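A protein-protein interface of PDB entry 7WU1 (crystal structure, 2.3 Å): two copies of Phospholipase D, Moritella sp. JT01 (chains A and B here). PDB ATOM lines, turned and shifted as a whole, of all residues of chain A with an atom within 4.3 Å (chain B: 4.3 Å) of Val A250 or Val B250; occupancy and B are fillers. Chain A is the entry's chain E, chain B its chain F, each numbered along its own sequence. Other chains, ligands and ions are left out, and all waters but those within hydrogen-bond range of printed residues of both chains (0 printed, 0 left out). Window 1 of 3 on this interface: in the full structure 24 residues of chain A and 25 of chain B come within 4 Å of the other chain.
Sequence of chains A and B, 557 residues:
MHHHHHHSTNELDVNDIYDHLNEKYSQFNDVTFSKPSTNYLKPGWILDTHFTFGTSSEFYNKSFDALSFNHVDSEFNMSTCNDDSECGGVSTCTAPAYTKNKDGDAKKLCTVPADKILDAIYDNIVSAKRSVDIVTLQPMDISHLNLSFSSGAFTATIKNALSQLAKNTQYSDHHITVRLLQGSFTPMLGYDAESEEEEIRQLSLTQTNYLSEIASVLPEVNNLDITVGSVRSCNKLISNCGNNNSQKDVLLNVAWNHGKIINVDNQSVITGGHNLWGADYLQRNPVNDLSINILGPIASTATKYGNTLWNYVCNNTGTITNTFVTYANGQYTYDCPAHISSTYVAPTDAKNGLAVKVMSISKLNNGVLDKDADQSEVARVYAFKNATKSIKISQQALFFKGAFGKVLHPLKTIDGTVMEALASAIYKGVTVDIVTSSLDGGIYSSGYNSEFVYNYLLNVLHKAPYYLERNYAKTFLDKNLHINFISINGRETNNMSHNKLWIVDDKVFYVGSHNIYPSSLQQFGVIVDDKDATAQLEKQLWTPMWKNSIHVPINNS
The backbone NH of Leu A237 sits at hydrogen-bond distance from the backbone carbonyl oxygen of Asn A253 (2.9 Å). The side-chain carboxylate of Asp A249 sits at hydrogen-bond distance from the backbone NH of Leu A251, 3.1 Å away. OD2 of Asp A249 is in hydrogen-bond range of N of Ala A403 (3.0 Å). The backbone NH of Leu B237 is in hydrogen-bond range of the backbone carbonyl oxygen of Asn B253 (2.7 Å). N of Leu B251 is in hydrogen-bond range of OD1 of Asp B249 (2.9 Å). N of Ala B403 is in hydrogen-bond range of OD1 of Asp B249, 2.9 Å away.
Val B250 touches Pro A187. Leu A237 touches Leu B237 (CD1 to O, 3.99 Å). CG2 of Val A250 touches CG of Pro B187, at 3.6 Å. CG2 of Val A250 touches CD1 of Leu B237, at 3.9 Å. CG1 of Val B250 touches CG1 of Val A250 (3.9 Å). Leu A251 touches Ala B403. Ala A403 touches Leu B251.
Val A250 touches just these residues of chain B: Pro B187, Leu B237 and Val B250. Val B250 touches two residues of chain A. Printed residues of chain A within 4 Å of Pro B187: Val A250. Of the printed residues of chain A, Leu B251 touches Ala A403. Of the printed residues of chain B, Leu A251 touches Ala B403 (3.6 Å). Printed residues of chain B within 4 Å of Ala A403: Leu B251 (3.6 Å). Leu A252 touches none of the printed residues of chain B. The nearest printed residue of chain A that does not touch Ala B403 is Val A250 (6.4 Å).
Of the 8 printed residues of chain A, 5 touch a printed residue of chain B. Printed residues of chain A that touch a printed residue of chain B: Pro A187, Leu A237, Val A250, Leu A251 and Ala A403. Hydrophobic or aromatic side chains of chain A that line the printed part of chain B: Pro A187, Leu A237, Val A250, Leu A251 and Ala A403. Printed residues of chain B that touch a printed residue of chain A: Pro B187, Leu B237, Val B250, Leu B251 and Ala B403.
Pro A187 touches Val B250, and with the chains exchanged Val A250 touches Pro B187. Val A250 touches Leu B237, but with the chains exchanged Leu A237 does not touch Val B250 (4.1 Å). Val B250 touches its own counterpart, Val A250. Leu A251 touches Ala B403, and with the chains exchanged Ala A403 touches Leu B251.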
ATOM      1  N   PRO A 187      17.612  -7.226   2.412  1.00  0.00           N
ATOM      2  CA  PRO A 187      17.504  -8.516   3.100  1.00  0.00           C
ATOM      3  C   PRO A 187      17.163  -8.356   4.566  1.00  0.00           C
ATOM      4  O   PRO A 187      17.590  -7.399   5.208  1.00  0.00           O
ATOM      5  CB  PRO A 187      18.893  -9.142   2.928  1.00  0.00           C
ATOM      6  CG  PRO A 187      19.799  -7.991   2.580  1.00  0.00           C
ATOM      7  CD  PRO A 187      18.935  -7.025   1.803  1.00  0.00           C
ATOM      8  N   LEU A 237      20.248  -4.568  -4.821  1.00  0.00           N
ATOM      9  CA  LEU A 237      21.523  -4.202  -4.216  1.00  0.00           C
ATOM     10  C   LEU A 237      22.554  -3.766  -5.255  1.00  0.00           C
ATOM     11  O   LEU A 237      23.288  -2.784  -5.033  1.00  0.00           O
ATOM     12  CB  LEU A 237      22.097  -5.360  -3.403  1.00  0.00           C
ATOM     13  CG  LEU A 237      21.395  -5.674  -2.089  1.00  0.00           C
ATOM     14  CD1 LEU A 237      21.918  -6.960  -1.481  1.00  0.00           C
ATOM     15  CD2 LEU A 237      21.513  -4.493  -1.095  1.00  0.00           C
ATOM     16  N   ASP A 249      24.574   4.125  -4.992  1.00  0.00           N
ATOM     17  CA  ASP A 249      25.044   3.548  -3.738  1.00  0.00           C
ATOM     18  C   ASP A 249      24.291   2.255  -3.482  1.00  0.00           C
ATOM     19  O   ASP A 249      23.111   2.143  -3.823  1.00  0.00           O
ATOM     20  CB  ASP A 249      24.850   4.522  -2.566  1.00  0.00           C
ATOM     21  CG  ASP A 249      25.678   4.145  -1.358  1.00  0.00           C
ATOM     22  OD1 ASP A 249      26.874   4.529  -1.303  1.00  0.00           O
ATOM     23  OD2 ASP A 249      25.131   3.448  -0.483  1.00  0.00           O
ATOM     24  N   VAL A 250      24.986   1.283  -2.890  1.00  0.00           N
ATOM     25  CA  VAL A 250      24.355  -0.001  -2.581  1.00  0.00           C
ATOM     26  C   VAL A 250      23.097   0.213  -1.750  1.00  0.00           C
ATOM     27  O   VAL A 250      22.084  -0.468  -1.941  1.00  0.00           O
ATOM     28  CB  VAL A 250      25.360  -0.921  -1.855  1.00  0.00           C
ATOM     29  CG1 VAL A 250      24.654  -2.122  -1.222  1.00  0.00           C
ATOM     30  CG2 VAL A 250      26.454  -1.369  -2.812  1.00  0.00           C
ATOM     31  N   LEU A 251      23.143   1.147  -0.801  1.00  0.00           N
ATOM     32  CA  LEU A 251      22.048   1.357   0.123  1.00  0.00           C
ATOM     33  C   LEU A 251      20.850   2.044  -0.507  1.00  0.00           C
ATOM     34  O   LEU A 251      19.763   2.010   0.083  1.00  0.00           O
ATOM     35  CB  LEU A 251      22.543   2.165   1.327  1.00  0.00           C
ATOM     36  CG  LEU A 251      23.582   1.424   2.167  1.00  0.00           C
ATOM     37  CD1 LEU A 251      23.937   2.202   3.426  1.00  0.00           C
ATOM     38  CD2 LEU A 251      23.120   0.004   2.550  1.00  0.00           C
ATOM     39  N   LEU A 252      21.018   2.646  -1.675  1.00  0.00           N
ATOM     40  CA  LEU A 252      19.888   3.129  -2.440  1.00  0.00           C
ATOM     41  C   LEU A 252      19.262   2.057  -3.329  1.00  0.00           C
ATOM     42  O   LEU A 252      18.233   2.316  -3.946  1.00  0.00           O
ATOM     43  CB  LEU A 252      20.320   4.300  -3.312  1.00  0.00           C
ATOM     44  CG  LEU A 252      20.767   5.522  -2.521  1.00  0.00           C
ATOM     45  CD1 LEU A 252      21.261   6.586  -3.502  1.00  0.00           C
ATOM     46  CD2 LEU A 252      19.690   6.106  -1.639  1.00  0.00           C
ATOM     47  N   ASN A 253      19.842   0.862  -3.405  1.00  0.00           N
ATOM     48  CA  ASN A 253      19.385  -0.161  -4.336  1.00  0.00           C
ATOM     49  C   ASN A 253      18.514  -1.231  -3.671  1.00  0.00           C
ATOM     50  O   ASN A 253      18.499  -2.400  -4.098  1.00  0.00           O
ATOM     51  CB  ASN A 253      20.595  -0.788  -5.027  1.00  0.00           C
ATOM     52  CG  ASN A 253      21.301   0.184  -5.946  1.00  0.00           C
ATOM     53  OD1 ASN A 253      20.760   1.226  -6.295  1.00  0.00           O
ATOM     54  ND2 ASN A 253      22.509  -0.154  -6.342  1.00  0.00           N
ATOM     55  N   ALA A 403      27.118   3.047   1.764  1.00  0.00           N
ATOM     56  CA  ALA A 403      27.592   1.741   2.199  1.00  0.00           C
ATOM     57  C   ALA A 403      29.050   1.759   2.639  1.00  0.00           C
ATOM     58  O   ALA A 403      29.447   1.015   3.546  1.00  0.00           O
ATOM     59  CB  ALA A 403      27.393   0.749   1.066  1.00  0.00           C
ATOM     60  N   PRO B 187      31.544  -2.195  -4.702  1.00  0.00           N
ATOM     61  CA  PRO B 187      31.556  -1.312  -5.885  1.00  0.00           C
ATOM     62  C   PRO B 187      32.157   0.050  -5.612  1.00  0.00           C
ATOM     63  O   PRO B 187      32.061   0.572  -4.499  1.00  0.00           O
ATOM     64  CB  PRO B 187      30.069  -1.170  -6.258  1.00  0.00           C
ATOM     65  CG  PRO B 187      29.306  -1.621  -5.010  1.00  0.00           C
ATOM     66  CD  PRO B 187      30.191  -2.677  -4.370  1.00  0.00           C
ATOM     67  N   LEU B 237      27.944  -9.028  -2.208  1.00  0.00           N
ATOM     68  CA  LEU B 237      26.884  -8.271  -1.561  1.00  0.00           C
ATOM     69  C   LEU B 237      25.687  -9.118  -1.134  1.00  0.00           C
ATOM     70  O   LEU B 237      25.104  -8.893  -0.063  1.00  0.00           O
ATOM     71  CB  LEU B 237      26.386  -7.164  -2.490  1.00  0.00           C
ATOM     72  CG  LEU B 237      27.306  -5.966  -2.724  1.00  0.00           C
ATOM     73  CD1 LEU B 237      26.790  -5.129  -3.914  1.00  0.00           C
ATOM     74  CD2 LEU B 237      27.438  -5.121  -1.489  1.00  0.00           C
ATOM     75  N   ASP B 249      25.301  -9.506   7.159  1.00  0.00           N
ATOM     76  CA  ASP B 249      24.927  -8.151   6.798  1.00  0.00           C
ATOM     77  C   ASP B 249      25.455  -7.881   5.397  1.00  0.00           C
ATOM     78  O   ASP B 249      26.473  -8.446   4.976  1.00  0.00           O
ATOM     79  CB  ASP B 249      25.463  -7.137   7.812  1.00  0.00           C
ATOM     80  CG  ASP B 249      24.806  -5.761   7.660  1.00  0.00           C
ATOM     81  OD1 ASP B 249      25.284  -4.975   6.796  1.00  0.00           O
ATOM     82  OD2 ASP B 249      23.798  -5.474   8.377  1.00  0.00           O
ATOM     83  N   VAL B 250      24.733  -7.026   4.671  1.00  0.00           N
ATOM     84  CA  VAL B 250      25.164  -6.646   3.328  1.00  0.00           C
ATOM     85  C   VAL B 250      26.585  -6.084   3.359  1.00  0.00           C
ATOM     86  O   VAL B 250      27.418  -6.396   2.500  1.00  0.00           O
ATOM     87  CB  VAL B 250      24.178  -5.625   2.732  1.00  0.00           C
ATOM     88  CG1 VAL B 250      24.781  -4.948   1.520  1.00  0.00           C
ATOM     89  CG2 VAL B 250      22.871  -6.265   2.416  1.00  0.00           C
ATOM     90  N   LEU B 251      26.889  -5.261   4.358  1.00  0.00           N
ATOM     91  CA  LEU B 251      28.185  -4.602   4.416  1.00  0.00           C
ATOM     92  C   LEU B 251      29.321  -5.554   4.753  1.00  0.00           C
ATOM     93  O   LEU B 251      30.485  -5.147   4.676  1.00  0.00           O
ATOM     94  CB  LEU B 251      28.142  -3.468   5.438  1.00  0.00           C
ATOM     95  CG  LEU B 251      27.126  -2.367   5.128  1.00  0.00           C
ATOM     96  CD1 LEU B 251      27.275  -1.184   6.124  1.00  0.00           C
ATOM     97  CD2 LEU B 251      27.248  -1.884   3.707  1.00  0.00           C
ATOM     98  N   LEU B 252      29.019  -6.787   5.145  1.00  0.00           N
ATOM     99  CA  LEU B 252      30.047  -7.802   5.335  1.00  0.00           C
ATOM    100  C   LEU B 252      30.252  -8.677   4.106  1.00  0.00           C
ATOM    101  O   LEU B 252      31.099  -9.581   4.131  1.00  0.00           O
ATOM    102  CB  LEU B 252      29.697  -8.698   6.520  1.00  0.00           C
ATOM    103  CG  LEU B 252      29.621  -8.030   7.888  1.00  0.00           C
ATOM    104  CD1 LEU B 252      29.115  -9.051   8.915  1.00  0.00           C
ATOM    105  CD2 LEU B 252      30.966  -7.477   8.301  1.00  0.00           C
ATOM    106  N   ASN B 253      29.499  -8.442   3.036  1.00  0.00           N
ATOM    107  CA  ASN B 253      29.556  -9.274   1.844  1.00  0.00           C
ATOM    108  C   ASN B 253      30.346  -8.614   0.719  1.00  0.00           C
ATOM    109  O   ASN B 253      30.054  -8.842  -0.461  1.00  0.00           O
ATOM    110  CB  ASN B 253      28.138  -9.628   1.405  1.00  0.00           C
ATOM    111  CG  ASN B 253      27.419 -10.512   2.442  1.00  0.00           C
ATOM    112  OD1 ASN B 253      28.060 -11.098   3.338  1.00  0.00           O
ATOM    113  ND2 ASN B 253      26.093 -10.619   2.320  1.00  0.00           N
ATOM    114  N   ALA B 403      24.089  -2.415   7.224  1.00  0.00           N
ATOM    115  CA  ALA B 403      23.472  -1.719   6.099  1.00  0.00           C
ATOM    116  C   ALA B 403      22.163  -1.037   6.468  1.00  0.00           C
ATOM    117  O   ALA B 403      21.850   0.031   5.930  1.00  0.00           O
ATOM    118  CB  ALA B 403      23.233  -2.697   4.959  1.00  0.00           C
